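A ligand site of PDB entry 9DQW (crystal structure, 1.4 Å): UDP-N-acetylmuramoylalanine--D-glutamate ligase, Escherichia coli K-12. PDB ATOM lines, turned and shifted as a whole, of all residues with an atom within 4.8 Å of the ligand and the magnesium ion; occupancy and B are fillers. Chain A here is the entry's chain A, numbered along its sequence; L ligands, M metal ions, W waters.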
ATOM      1  N   ILE A  12      14.644 -18.705 -13.608  1.00  0.00           N
ATOM      2  CA  ILE A  12      15.677 -17.835 -14.171  1.00  0.00           C
ATOM      3  C   ILE A  12      15.372 -16.394 -13.772  1.00  0.00           C
ATOM      4  O   ILE A  12      14.303 -15.860 -14.094  1.00  0.00           O
ATOM      5  CB  ILE A  12      15.753 -17.930 -15.688  1.00  0.00           C
ATOM      6  CG1 ILE A  12      15.957 -19.370 -16.161  1.00  0.00           C
ATOM      7  CG2 ILE A  12      16.901 -17.009 -16.170  1.00  0.00           C
ATOM      8  CD1 ILE A  12      15.842 -19.541 -17.670  1.00  0.00           C
ATOM      9  N   GLY A  13      16.315 -15.778 -13.081  1.00  0.00           N
ATOM     10  CA  GLY A  13      16.230 -14.401 -12.676  1.00  0.00           C
ATOM     11  C   GLY A  13      16.131 -14.278 -11.170  1.00  0.00           C
ATOM     12  O   GLY A  13      15.217 -14.826 -10.549  1.00  0.00           O
ATOM     13  N   GLY A  15      15.676 -11.417  -9.397  1.00  0.00           N
ATOM     14  CA  GLY A  15      15.139 -10.109  -9.083  1.00  0.00           C
ATOM     15  C   GLY A  15      13.799 -10.241  -8.392  1.00  0.00           C
ATOM     16  O   GLY A  15      13.539 -11.286  -7.774  1.00  0.00           O
ATOM     17  N   LEU A  16      12.948  -9.230  -8.529  1.00  0.00           N
ATOM     18  CA  LEU A  16      11.661  -9.219  -7.845  1.00  0.00           C
ATOM     19  C   LEU A  16      10.818 -10.403  -8.265  1.00  0.00           C
ATOM     20  O   LEU A  16      10.202 -11.079  -7.423  1.00  0.00           O
ATOM     21  CB  LEU A  16      10.883  -7.945  -8.182  1.00  0.00           C
ATOM     22  CG  LEU A  16      11.415  -6.607  -7.723  1.00  0.00           C
ATOM     23  CD1 LEU A  16      10.468  -5.513  -8.254  1.00  0.00           C
ATOM     24  CD2 LEU A  16      11.507  -6.563  -6.209  1.00  0.00           C
ATOM     25  N   THR A  17      10.741 -10.633  -9.572  1.00  0.00           N
ATOM     26  CA  THR A  17       9.914 -11.734 -10.062  1.00  0.00           C
ATOM     27  C   THR A  17      10.440 -13.062  -9.566  1.00  0.00           C
ATOM     28  O   THR A  17       9.676 -13.897  -9.060  1.00  0.00           O
ATOM     29  CB  THR A  17       9.875 -11.714 -11.598  1.00  0.00           C
ATOM     30  OG1 THR A  17       9.337 -10.485 -12.048  1.00  0.00           O
ATOM     31  CG2 THR A  17       9.011 -12.861 -12.095  1.00  0.00           C
ATOM     32  N   GLY A  18      11.742 -13.301  -9.716  1.00  0.00           N
ATOM     33  CA  GLY A  18      12.282 -14.592  -9.346  1.00  0.00           C
ATOM     34  C   GLY A  18      12.078 -14.903  -7.875  1.00  0.00           C
ATOM     35  O   GLY A  18      11.757 -16.030  -7.509  1.00  0.00           O
ATOM     36  N   MET A  35      18.709 -19.537 -11.091  1.00  0.00           N
ATOM     37  CA  MET A  35      19.906 -19.083 -11.780  1.00  0.00           C
ATOM     38  C   MET A  35      19.725 -17.684 -12.345  1.00  0.00           C
ATOM     39  O   MET A  35      18.611 -17.203 -12.548  1.00  0.00           O
ATOM     40  CB  MET A  35      20.291 -20.030 -12.912  1.00  0.00           C
ATOM     41  CG  MET A  35      19.309 -20.044 -14.046  1.00  0.00           C
ATOM     42  SD  MET A  35      19.688 -21.206 -15.350  1.00  0.00           S
ATOM     43  CE  MET A  35      19.676 -22.732 -14.460  1.00  0.00           C
ATOM     44  N   ASP A  36      20.847 -17.009 -12.615  1.00  0.00           N
ATOM     45  CA  ASP A  36      20.821 -15.663 -13.187  1.00  0.00           C
ATOM     46  C   ASP A  36      22.131 -15.477 -13.941  1.00  0.00           C
ATOM     47  O   ASP A  36      23.182 -15.921 -13.464  1.00  0.00           O
ATOM     48  CB  ASP A  36      20.704 -14.638 -12.044  1.00  0.00           C
ATOM     49  CG  ASP A  36      20.345 -13.231 -12.525  1.00  0.00           C
ATOM     50  OD1 ASP A  36      21.169 -12.570 -13.188  1.00  0.00           O
ATOM     51  OD2 ASP A  36      19.227 -12.766 -12.198  1.00  0.00           O
ATOM     52  N   THR A  37      22.092 -14.787 -15.107  1.00  0.00           N
ATOM     53  CA  THR A  37      23.332 -14.564 -15.848  1.00  0.00           C
ATOM     54  C   THR A  37      24.276 -13.589 -15.164  1.00  0.00           C
ATOM     55  O   THR A  37      25.482 -13.603 -15.458  1.00  0.00           O
ATOM     56  CB  THR A  37      23.057 -14.079 -17.267  1.00  0.00           C
ATOM     57  OG1 THR A  37      22.470 -12.778 -17.217  1.00  0.00           O
ATOM     58  CG2 THR A  37      22.157 -15.028 -18.014  1.00  0.00           C
ATOM     59  N   ARG A  38      23.783 -12.735 -14.272  1.00  0.00           N
ATOM     60  CA  ARG A  38      24.629 -11.764 -13.609  1.00  0.00           C
ATOM     61  C   ARG A  38      25.380 -12.436 -12.474  1.00  0.00           C
ATOM     62  O   ARG A  38      24.851 -13.331 -11.803  1.00  0.00           O
ATOM     63  CB  ARG A  38      23.776 -10.633 -13.069  1.00  0.00           C
ATOM     64  CG  ARG A  38      23.144  -9.822 -14.165  1.00  0.00           C
ATOM     65  CD  ARG A  38      22.060  -8.929 -13.616  1.00  0.00           C
ATOM     66  NE  ARG A  38      20.911  -9.700 -13.182  1.00  0.00           N
ATOM     67  CZ  ARG A  38      19.801  -9.161 -12.701  1.00  0.00           C
ATOM     68  NH1 ARG A  38      19.663  -7.848 -12.594  1.00  0.00           N
ATOM     69  NH2 ARG A  38      18.798  -9.951 -12.325  1.00  0.00           N
ATOM     70  N   LEU A  58      23.777 -18.867 -17.400  1.00  0.00           N
ATOM     71  CA  LEU A  58      22.747 -19.895 -17.285  1.00  0.00           C
ATOM     72  C   LEU A  58      23.405 -21.270 -17.217  1.00  0.00           C
ATOM     73  O   LEU A  58      24.399 -21.530 -17.885  1.00  0.00           O
ATOM     74  CB  LEU A  58      21.732 -19.823 -18.422  1.00  0.00           C
ATOM     75  CG  LEU A  58      20.961 -18.494 -18.540  1.00  0.00           C
ATOM     76  CD1 LEU A  58      19.823 -18.616 -19.529  1.00  0.00           C
ATOM     77  CD2 LEU A  58      20.426 -18.020 -17.193  1.00  0.00           C
ATOM     78  N   SER A  72      11.883 -15.235 -15.616  1.00  0.00           N
ATOM     79  CA  SER A  72      11.588 -13.850 -15.324  1.00  0.00           C
ATOM     80  C   SER A  72      11.472 -13.073 -16.638  1.00  0.00           C
ATOM     81  O   SER A  72      12.092 -13.451 -17.647  1.00  0.00           O
ATOM     82  CB  SER A  72      12.698 -13.246 -14.467  1.00  0.00           C
ATOM     83  OG  SER A  72      12.721 -13.824 -13.156  1.00  0.00           O
ATOM     84  N   PRO A  73      10.719 -11.977 -16.664  1.00  0.00           N
ATOM     85  CA  PRO A  73      10.570 -11.234 -17.920  1.00  0.00           C
ATOM     86  C   PRO A  73      11.860 -10.648 -18.460  1.00  0.00           C
ATOM     87  O   PRO A  73      11.940 -10.402 -19.667  1.00  0.00           O
ATOM     88  CB  PRO A  73       9.548 -10.149 -17.579  1.00  0.00           C
ATOM     89  CG  PRO A  73       9.643  -9.989 -16.095  1.00  0.00           C
ATOM     90  CD  PRO A  73       9.924 -11.375 -15.576  1.00  0.00           C
ATOM     91  N   GLY A  74      12.859 -10.420 -17.623  1.00  0.00           N
ATOM     92  CA  GLY A  74      14.126  -9.865 -18.032  1.00  0.00           C
ATOM     93  C   GLY A  74      15.060 -10.817 -18.746  1.00  0.00           C
ATOM     94  O   GLY A  74      16.114 -10.356 -19.204  1.00  0.00           O
ATOM     95  N   ILE A  75      14.762 -12.105 -18.860  1.00  0.00           N
ATOM     96  CA  ILE A  75      15.575 -13.015 -19.670  1.00  0.00           C
ATOM     97  C   ILE A  75      14.852 -13.266 -21.000  1.00  0.00           C
ATOM     98  O   ILE A  75      13.671 -13.597 -21.029  1.00  0.00           O
ATOM     99  CB  ILE A  75      15.908 -14.317 -18.919  1.00  0.00           C
ATOM    100  CG1 ILE A  75      16.998 -15.115 -19.655  1.00  0.00           C
ATOM    101  CG2 ILE A  75      14.704 -15.203 -18.718  1.00  0.00           C
ATOM    102  CD1 ILE A  75      18.401 -14.579 -19.477  1.00  0.00           C
ATOM    103  N   ASP A  95       5.900 -15.844 -14.417  1.00  0.00           N
ATOM    104  CA  ASP A  95       5.094 -15.678 -13.210  1.00  0.00           C
ATOM    105  C   ASP A  95       3.634 -15.378 -13.525  1.00  0.00           C
ATOM    106  O   ASP A  95       2.747 -15.804 -12.780  1.00  0.00           O
ATOM    107  CB  ASP A  95       5.695 -14.624 -12.253  1.00  0.00           C
ATOM    108  CG  ASP A  95       5.595 -13.186 -12.766  1.00  0.00           C
ATOM    109  OD1 ASP A  95       5.964 -12.913 -13.940  1.00  0.00           O
ATOM    110  OD2 ASP A  95       5.229 -12.306 -11.976  1.00  0.00           O
ATOM    111  N   LYS A 116       0.152   2.348 -19.200  1.00  0.00           N
ATOM    112  CA  LYS A 116      -0.311   1.111 -18.562  1.00  0.00           C
ATOM    113  C   LYS A 116      -0.535   1.273 -17.063  1.00  0.00           C
ATOM    114  O   LYS A 116      -1.551   0.809 -16.523  1.00  0.00           O
ATOM    115  CB  LYS A 116       0.728  -0.009 -18.759  1.00  0.00           C
ATOM    116  CG  LYS A 116       0.961  -0.493 -20.132  1.00  0.00           C
ATOM    117  CD  LYS A 116       1.868  -1.747 -20.096  1.00  0.00           C
ATOM    118  CE  LYS A 116       3.280  -1.504 -19.604  1.00  0.00           C
ATOM    119  NZ  LYS A 116       4.029  -0.564 -20.485  1.00  0.00           N
ATOM    120  N   GLY A 138       1.379  -6.853 -11.094  1.00  0.00           N
ATOM    121  CA  GLY A 138       2.073  -7.127 -12.331  1.00  0.00           C
ATOM    122  C   GLY A 138       3.237  -6.202 -12.577  1.00  0.00           C
ATOM    123  O   GLY A 138       3.976  -5.837 -11.647  1.00  0.00           O
ATOM    124  N   ASN A 139       3.411  -5.780 -13.832  1.00  0.00           N
ATOM    125  CA  ASN A 139       4.546  -4.964 -14.224  1.00  0.00           C
ATOM    126  C   ASN A 139       4.584  -3.610 -13.535  1.00  0.00           C
ATOM    127  O   ASN A 139       5.644  -2.975 -13.492  1.00  0.00           O
ATOM    128  CB  ASN A 139       4.488  -4.786 -15.745  1.00  0.00           C
ATOM    129  CG  ASN A 139       5.754  -4.179 -16.328  1.00  0.00           C
ATOM    130  OD1 ASN A 139       6.818  -4.806 -16.338  1.00  0.00           O
ATOM    131  ND2 ASN A 139       5.643  -2.959 -16.832  1.00  0.00           N
ATOM    132  N   ILE A 140       3.462  -3.167 -12.954  1.00  0.00           N
ATOM    133  CA  ILE A 140       3.415  -1.954 -12.154  1.00  0.00           C
ATOM    134  C   ILE A 140       4.338  -2.011 -10.941  1.00  0.00           C
ATOM    135  O   ILE A 140       4.727  -0.964 -10.405  1.00  0.00           O
ATOM    136  CB  ILE A 140       1.949  -1.690 -11.784  1.00  0.00           C
ATOM    137  CG1 ILE A 140       1.789  -0.280 -11.255  1.00  0.00           C
ATOM    138  CG2 ILE A 140       1.448  -2.734 -10.780  1.00  0.00           C
ATOM    139  CD1 ILE A 140       0.316   0.140 -11.163  1.00  0.00           C
ATOM    140  N   GLY A 141       4.712  -3.208 -10.490  1.00  0.00           N
ATOM    141  CA  GLY A 141       5.759  -3.330  -9.480  1.00  0.00           C
ATOM    142  C   GLY A 141       5.460  -4.216  -8.298  1.00  0.00           C
ATOM    143  O   GLY A 141       6.338  -4.419  -7.456  1.00  0.00           O
ATOM    144  N   PRO A 143       4.647  -7.957  -7.701  1.00  0.00           N
ATOM    145  CA  PRO A 143       4.585  -9.201  -8.484  1.00  0.00           C
ATOM    146  C   PRO A 143       3.252  -9.913  -8.304  1.00  0.00           C
ATOM    147  O   PRO A 143       2.743 -10.051  -7.193  1.00  0.00           O
ATOM    148  CB  PRO A 143       5.741 -10.019  -7.895  1.00  0.00           C
ATOM    149  CG  PRO A 143       6.718  -8.977  -7.378  1.00  0.00           C
ATOM    150  CD  PRO A 143       5.821  -7.907  -6.819  1.00  0.00           C
ATOM    151  N   SER A 160       3.556  -6.534 -19.333  1.00  0.00           N
ATOM    152  CA  SER A 160       4.499  -6.124 -20.359  1.00  0.00           C
ATOM    153  C   SER A 160       4.495  -7.106 -21.522  1.00  0.00           C
ATOM    154  O   SER A 160       4.034  -8.248 -21.400  1.00  0.00           O
ATOM    155  CB  SER A 160       5.923  -6.073 -19.791  1.00  0.00           C
ATOM    156  OG  SER A 160       6.376  -7.385 -19.449  1.00  0.00           O
ATOM    157  N   PHE A 162       7.129  -8.605 -22.461  1.00  0.00           N
ATOM    158  CA  PHE A 162       7.953  -9.720 -22.017  1.00  0.00           C
ATOM    159  C   PHE A 162       7.128 -10.742 -21.247  1.00  0.00           C
ATOM    160  O   PHE A 162       7.275 -11.962 -21.432  1.00  0.00           O
ATOM    161  CB  PHE A 162       9.076  -9.234 -21.094  1.00  0.00           C
ATOM    162  CG  PHE A 162      10.003  -8.216 -21.691  1.00  0.00           C
ATOM    163  CD1 PHE A 162      10.286  -8.161 -23.044  1.00  0.00           C
ATOM    164  CD2 PHE A 162      10.659  -7.323 -20.844  1.00  0.00           C
ATOM    165  CE1 PHE A 162      11.160  -7.224 -23.553  1.00  0.00           C
ATOM    166  CE2 PHE A 162      11.522  -6.379 -21.348  1.00  0.00           C
ATOM    167  CZ  PHE A 162      11.794  -6.335 -22.707  1.00  0.00           C
ATOM    168  N   GLN A 163       6.269 -10.271 -20.345  1.00  0.00           N
ATOM    169  CA  GLN A 163       5.442 -11.181 -19.570  1.00  0.00           C
ATOM    170  C   GLN A 163       4.479 -11.937 -20.478  1.00  0.00           C
ATOM    171  O   GLN A 163       4.230 -13.141 -20.292  1.00  0.00           O
ATOM    172  CB  GLN A 163       4.654 -10.398 -18.522  1.00  0.00           C
ATOM    173  CG  GLN A 163       5.499  -9.922 -17.350  1.00  0.00           C
ATOM    174  CD  GLN A 163       4.813  -8.860 -16.504  1.00  0.00           C
ATOM    175  OE1 GLN A 163       4.014  -8.051 -17.005  1.00  0.00           O
ATOM    176  NE2 GLN A 163       5.113  -8.853 -15.220  1.00  0.00           N
ATOM    177  N   ASP A 183       9.644   0.269 -28.552  1.00  0.00           N
ATOM    178  CA  ASP A 183      10.287   0.099 -27.246  1.00  0.00           C
ATOM    179  C   ASP A 183      10.906  -1.294 -27.248  1.00  0.00           C
ATOM    180  O   ASP A 183      10.530  -2.164 -28.036  1.00  0.00           O
ATOM    181  CB  ASP A 183       9.274   0.266 -26.098  1.00  0.00           C
ATOM    182  CG  ASP A 183       9.912   0.528 -24.728  1.00  0.00           C
ATOM    183  OD1 ASP A 183      11.170   0.622 -24.579  1.00  0.00           O
ATOM    184  OD2 ASP A 183       9.107   0.726 -23.775  1.00  0.00           O
ATOM    185  N   HIS A 184      11.849  -1.494 -26.337  1.00  0.00           N
ATOM    186  CA  HIS A 184      12.453  -2.806 -26.108  1.00  0.00           C
ATOM    187  C   HIS A 184      13.072  -3.431 -27.347  1.00  0.00           C
ATOM    188  O   HIS A 184      13.105  -4.659 -27.467  1.00  0.00           O
ATOM    189  CB  HIS A 184      11.426  -3.752 -25.495  1.00  0.00           C
ATOM    190  CG  HIS A 184      10.840  -3.216 -24.232  1.00  0.00           C
ATOM    191  ND1 HIS A 184      11.620  -2.946 -23.137  1.00  0.00           N
ATOM    192  CD2 HIS A 184       9.576  -2.880 -23.897  1.00  0.00           C
ATOM    193  CE1 HIS A 184      10.847  -2.468 -22.164  1.00  0.00           C
ATOM    194  NE2 HIS A 184       9.603  -2.412 -22.601  1.00  0.00           N
ATOM    195  N   KCX A 199       2.391  -8.317 -27.589  1.00  0.00           N
ATOM    196  CA  KCX A 199       1.260  -7.646 -26.961  1.00  0.00           C
ATOM    197  CB  KCX A 199       1.299  -6.151 -27.237  1.00  0.00           C
ATOM    198  CG  KCX A 199       2.470  -5.448 -26.592  1.00  0.00           C
ATOM    199  CD  KCX A 199       2.292  -3.924 -26.513  1.00  0.00           C
ATOM    200  CE  KCX A 199       3.434  -3.204 -25.799  1.00  0.00           C
ATOM    201  NZ  KCX A 199       3.600  -3.581 -24.414  1.00  0.00           N
ATOM    202  C   KCX A 199      -0.080  -8.209 -27.411  1.00  0.00           C
ATOM    203  O   KCX A 199      -1.015  -8.291 -26.618  1.00  0.00           O
ATOM    204  CX  KCX A 199       4.653  -3.139 -23.571  1.00  0.00           C
ATOM    205  OQ1 KCX A 199       4.710  -3.592 -22.392  1.00  0.00           O
ATOM    206  OQ2 KCX A 199       5.471  -2.307 -24.058  1.00  0.00           O
ATOM    207  N   THR A 322      10.256   6.028 -20.140  1.00  0.00           N
ATOM    208  CA  THR A 322      11.346   5.117 -20.462  1.00  0.00           C
ATOM    209  C   THR A 322      11.409   4.779 -21.938  1.00  0.00           C
ATOM    210  O   THR A 322      12.156   3.876 -22.321  1.00  0.00           O
ATOM    211  CB  THR A 322      11.173   3.839 -19.651  1.00  0.00           C
ATOM    212  OG1 THR A 322       9.838   3.339 -19.859  1.00  0.00           O
ATOM    213  CG2 THR A 322      11.410   4.145 -18.150  1.00  0.00           C
ATOM    214  N   LEU A 417      18.489   1.254 -15.877  1.00  0.00           N
ATOM    215  CA  LEU A 417      19.258   0.215 -15.217  1.00  0.00           C
ATOM    216  C   LEU A 417      20.758   0.282 -15.489  1.00  0.00           C
ATOM    217  O   LEU A 417      21.498  -0.480 -14.871  1.00  0.00           O
ATOM    218  CB  LEU A 417      18.727  -1.186 -15.581  1.00  0.00           C
ATOM    219  CG  LEU A 417      17.231  -1.423 -15.262  1.00  0.00           C
ATOM    220  CD1 LEU A 417      16.880  -2.885 -15.535  1.00  0.00           C
ATOM    221  CD2 LEU A 417      16.856  -1.072 -13.850  1.00  0.00           C
ATOM    222  N   PHE A 423      13.614   2.840 -11.957  1.00  0.00           N
ATOM    223  CA  PHE A 423      13.260   4.197 -12.355  1.00  0.00           C
ATOM    224  C   PHE A 423      12.797   5.011 -11.170  1.00  0.00           C
ATOM    225  O   PHE A 423      12.866   6.247 -11.217  1.00  0.00           O
ATOM    226  CB  PHE A 423      12.214   4.212 -13.491  1.00  0.00           C
ATOM    227  CG  PHE A 423      10.840   3.769 -13.061  1.00  0.00           C
ATOM    228  CD1 PHE A 423       9.989   4.647 -12.377  1.00  0.00           C
ATOM    229  CD2 PHE A 423      10.398   2.480 -13.295  1.00  0.00           C
ATOM    230  CE1 PHE A 423       8.743   4.227 -11.950  1.00  0.00           C
ATOM    231  CE2 PHE A 423       9.137   2.068 -12.872  1.00  0.00           C
ATOM    232  CZ  PHE A 423       8.317   2.952 -12.191  1.00  0.00           C
HETATM  233  N1  LIG L   1      18.681  -9.935 -15.997  1.00  0.00           N
HETATM  234  C1  LIG L   1      19.904 -10.467 -16.375  1.00  0.00           C
HETATM  235  N2  LIG L   1      20.000 -11.817 -16.244  1.00  0.00           N
HETATM  236  C2  LIG L   1      19.060 -12.699 -15.779  1.00  0.00           C
HETATM  237  C3  LIG L   1      17.818 -12.076 -15.421  1.00  0.00           C
HETATM  238  C4  LIG L   1      17.674 -10.746 -15.542  1.00  0.00           C
HETATM  239  O1  LIG L   1      20.812  -9.779 -16.811  1.00  0.00           O
HETATM  240  O2  LIG L   1      19.307 -13.904 -15.689  1.00  0.00           O
HETATM  241  C5  LIG L   1      18.410  -8.524 -16.133  1.00  0.00           C
HETATM  242  C6  LIG L   1      17.429  -8.230 -17.277  1.00  0.00           C
HETATM  243  O3  LIG L   1      18.039  -8.119 -18.525  1.00  0.00           O
HETATM  244  C7  LIG L   1      16.754  -6.940 -16.856  1.00  0.00           C
HETATM  245  C8  LIG L   1      16.897  -6.979 -15.347  1.00  0.00           C
HETATM  246  O4  LIG L   1      17.782  -8.061 -14.997  1.00  0.00           O
HETATM  247  O5  LIG L   1      17.416  -5.839 -17.426  1.00  0.00           O
HETATM  248  C9  LIG L   1      15.569  -7.131 -14.640  1.00  0.00           C
HETATM  249  O6  LIG L   1      14.959  -8.342 -15.080  1.00  0.00           O
HETATM  250  P1  LIG L   1      14.003  -9.155 -14.043  1.00  0.00           P
HETATM  251  O7  LIG L   1      13.134 -10.060 -14.847  1.00  0.00           O
HETATM  252  O8  LIG L   1      14.803  -9.685 -12.902  1.00  0.00           O
HETATM  253  O9  LIG L   1      13.144  -7.917 -13.462  1.00  0.00           O
HETATM  254  P2  LIG L   1      12.312  -7.880 -12.083  1.00  0.00           P
HETATM  255  O10 LIG L   1      11.696  -9.160 -11.729  1.00  0.00           O
HETATM  256  O11 LIG L   1      13.139  -7.186 -11.036  1.00  0.00           O
HETATM  257  O12 LIG L   1      11.162  -6.822 -12.533  1.00  0.00           O
HETATM  258  C10 LIG L   1      10.214  -7.265 -13.468  1.00  0.00           C
HETATM  259  C11 LIG L   1       9.948  -6.107 -14.444  1.00  0.00           C
HETATM  260  N3  LIG L   1      11.154  -5.801 -15.166  1.00  0.00           N
HETATM  261  C12 LIG L   1      11.318  -6.176 -16.437  1.00  0.00           C
HETATM  262  O13 LIG L   1      10.485  -6.810 -17.070  1.00  0.00           O
HETATM  263  C13 LIG L   1      12.630  -5.773 -17.050  1.00  0.00           C
HETATM  264  C14 LIG L   1       9.374  -4.948 -13.646  1.00  0.00           C
HETATM  265  O14 LIG L   1       8.979  -3.874 -14.455  1.00  0.00           O
HETATM  266  C15 LIG L   1       8.124  -5.443 -12.944  1.00  0.00           C
HETATM  267  O15 LIG L   1       7.567  -4.438 -12.116  1.00  0.00           O
HETATM  268  C16 LIG L   1       8.395  -6.680 -12.073  1.00  0.00           C
HETATM  269  O16 LIG L   1       9.048  -7.676 -12.835  1.00  0.00           O
HETATM  270  C17 LIG L   1       7.126  -7.312 -11.534  1.00  0.00           C
HETATM  271  O17 LIG L   1       6.319  -7.862 -12.561  1.00  0.00           O
HETATM  272  C18 LIG L   1       9.946  -2.875 -14.674  1.00  0.00           C
HETATM  273  C19 LIG L   1      10.203  -2.656 -16.151  1.00  0.00           C
HETATM  274  O18 LIG L   1      11.106  -1.922 -16.550  1.00  0.00           O
HETATM  275  C20 LIG L   1       9.418  -1.543 -14.132  1.00  0.00           C
HETATM  276  N4  LIG L   1       9.401  -3.289 -16.986  1.00  0.00           N
HETATM  277  C21 LIG L   1       9.534  -3.109 -18.407  1.00  0.00           C
HETATM  278  C22 LIG L   1       8.828  -1.813 -18.821  1.00  0.00           C
HETATM  279  O19 LIG L   1       9.218  -1.276 -19.862  1.00  0.00           O
HETATM  280  O20 LIG L   1       7.927  -1.320 -18.075  1.00  0.00           O
HETATM  281  C23 LIG L   1       8.984  -4.287 -19.194  1.00  0.00           C
HETATM  282 MG    MG M   1       8.105  -1.181 -21.327  1.00  0.00          MG
HETATM  283  O   HOH W   1      20.027  -5.007 -15.987  1.00  0.00           O
HETATM  284  O   HOH W   2       4.224  -9.766 -11.880  1.00  0.00           O
HETATM  285  O   HOH W   3      12.452  -0.362 -19.832  1.00  0.00           O
HETATM  286  O   HOH W   4       8.188  -5.590 -22.297  1.00  0.00           O
HETATM  287  O   HOH W   5       6.748  -2.824 -21.186  1.00  0.00           O
HETATM  288  O   HOH W   6       9.858   1.025 -21.144  1.00  0.00           O
HETATM  289  O   HOH W   7       6.829   0.292 -19.783  1.00  0.00           O
HETATM  290  O   HOH W   8       6.882  -0.661 -22.913  1.00  0.00           O
HETATM  291  O   HOH W   9       9.327  -2.944 -10.476  1.00  0.00           O
HETATM  292  O   HOH W  10      13.616  -1.920 -15.991  1.00  0.00           O
HETATM  293  O   HOH W  11      11.393   0.605 -17.527  1.00  0.00           O
HETATM  294  O   HOH W  12       8.738   1.460 -17.862  1.00  0.00           O
HETATM  295  O   HOH W  13      16.050  -7.918 -21.125  1.00  0.00           O
HETATM  296  O   HOH W  14      13.677 -11.850 -11.356  1.00  0.00           O
HETATM  297  O   HOH W  15       7.153 -10.374 -13.712  1.00  0.00           O
HETATM  298  O   HOH W  16      15.166  -6.874  -9.547  1.00  0.00           O
HETATM  299  O   HOH W  17      16.629  -8.323 -11.508  1.00  0.00           O
HETATM  300  O   HOH W  18       7.737  -7.209 -17.171  1.00  0.00           O
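The magnesium ion is bound by an oxygen (O19) of the ligand (1.8 Å). Water W8 binds the magnesium ion (2.1 Å). Water W5 is bound to the magnesium ion (2.1 Å). A ring nitrogen (NE2) of His 184 binds the magnesium ion (2.3 Å). The magnesium ion is bound by water W7 (2.5 Å). The magnesium ion has five donor atoms within binding distance. Slightly farther from the magnesium ion lies water W6 (2.8 Å).
The side-chain amide oxygen (OD1) of Asn 139 sits close to an oxygen (O14) of the ligand (3.0 Å). The side-chain amide nitrogen of Gln 163 is in hydrogen-bond range of an oxygen (O17) of the ligand (3.1 Å). The backbone carbonyl oxygen (O) of Asn 139 is in hydrogen-bond range of an oxygen (O15) of the ligand, at 2.8 Å. An oxygen (O7) of the ligand sits at hydrogen-bond distance from the backbone NH (N) of Gly 74, 2.8 Å away. N of Thr 17 sits at hydrogen-bond distance from O10 of the ligand (2.8 Å). The backbone NH of Leu 16 sits at hydrogen-bond distance from an oxygen (O11) of the ligand, 3.2 Å away. An oxygen (O3) of the ligand lies within hydrogen-bond range of the backbone carbonyl oxygen (O) of Gly 74 (3.0 Å). OG1 of Thr 37 sits at hydrogen-bond distance from N2 of the ligand (2.8 Å). The side-chain hydroxyl (OG1) of Thr 17 is in hydrogen-bond range of an oxygen (O10) of the ligand, at 2.7 Å. N of Thr 37 is in hydrogen-bond range of O2 of the ligand, 3.0 Å away. The side-chain carboxylate of Asp 36 sits close to a nitrogen (N2) of the ligand (3.4 Å). O of Gly 138 lies within hydrogen-bond range of O17 of the ligand. NH1 of Arg 38 sits at hydrogen-bond distance from O4 of the ligand.
Merely in contact with the magnesium ion: Asp 183 (3.3 Å) and KCX 199 (3.96 Å). Of the 31 residues printed, 3 come within 4 Å of the magnesium ion. The nearest printed residue that does not touch the magnesium ion is Lys 116 (4.2 Å).
The side-chain amide oxygen (OE1) of Gln 163 lies within hydrogen-bond range of the backbone NH (N) of Ser 160, at 2.8 Å. OG of Ser 72 is in hydrogen-bond range of O of Ile 12 (2.7 Å). OG of Ser 160 sits close to N of Phe 162 (3.3 Å). The backbone NH of Gly 13 lies within hydrogen-bond range of the backbone carbonyl oxygen of Met 35, 2.8 Å away. OQ1 of KCX 199 is in salt-bridge range of the side-chain amino group of Lys 116 (3.6 Å). NE2 of His 184 lies close to OD2 of Asp 183. OD2 of Asp 36 is in salt-bridge range of NH2 of Arg 38, 2.9 Å away.
Water W7 bridges an oxygen (O20) of the ligand (2.6 Å) and the side-chain amino group (NZ) of Lys 116 (3.0 Å). Water W8 lies within hydrogen-bond range of OQ2 of KCX 199 (2.5 Å) and OD2 of Asp 183 (2.8 Å). Water W16 bridges O11 of the ligand and N of Leu 16. Water W15 lies within hydrogen-bond range of the side-chain hydroxyl of Thr 17, the side-chain carboxylate of Asp 95, an oxygen (O17) of the ligand and the side-chain amide nitrogen of Gln 163. Water W14 lies within hydrogen-bond range of N of Gly 15 (2.8 Å), OG of Ser 72 (2.8 Å), O8 of the ligand (2.9 Å), N of Gly 18 (2.9 Å) and O of Gly 13 (3.4 Å). Water W12 lies within hydrogen-bond range of an oxygen (O20) of the ligand (2.9 Å) and the side-chain hydroxyl of Thr 322 (3.0 Å).
Ile 12 touches the ligand (CG2 to O2, 3.96 Å). Gly 13 touches the ligand (CA to C3, 3.9 Å). CA of Gly 15 touches O8 of the ligand (3.9 Å). Ser 72 touches the ligand. Pro 73 touches the ligand. CD1 of Ile 75 touches O2 of the ligand, at 3.95 Å. Gly 141 touches the ligand. CB of Ser 160 touches C23 of the ligand (3.6 Å). CD2 of Phe 162 touches O13 of the ligand, 3.8 Å away. Leu 417 touches the ligand (CD1 to O5, 3.5 Å). Phe 423 touches the ligand (CE2 to C20, 3.8 Å). Hydrophobic or aromatic side chains that line the ligand: Ile 12, Leu 16, Pro 73, Ile 75, Phe 162, His 184, Leu 417 and Phe 423. Within 4 Å of the ligand: Ile 12, Gly 13, Gly 15, Leu 16, Thr 17, Asp 36, Thr 37, Arg 38, Ser 72, Pro 73, Gly 74, Ile 75, Gly 138, Asn 139, Gly 141, Ser 160, Phe 162, Gln 163, His 184, Leu 417 and Phe 423. The nearest printed residue that does not touch the ligand is Ile 140 (4.2 Å).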
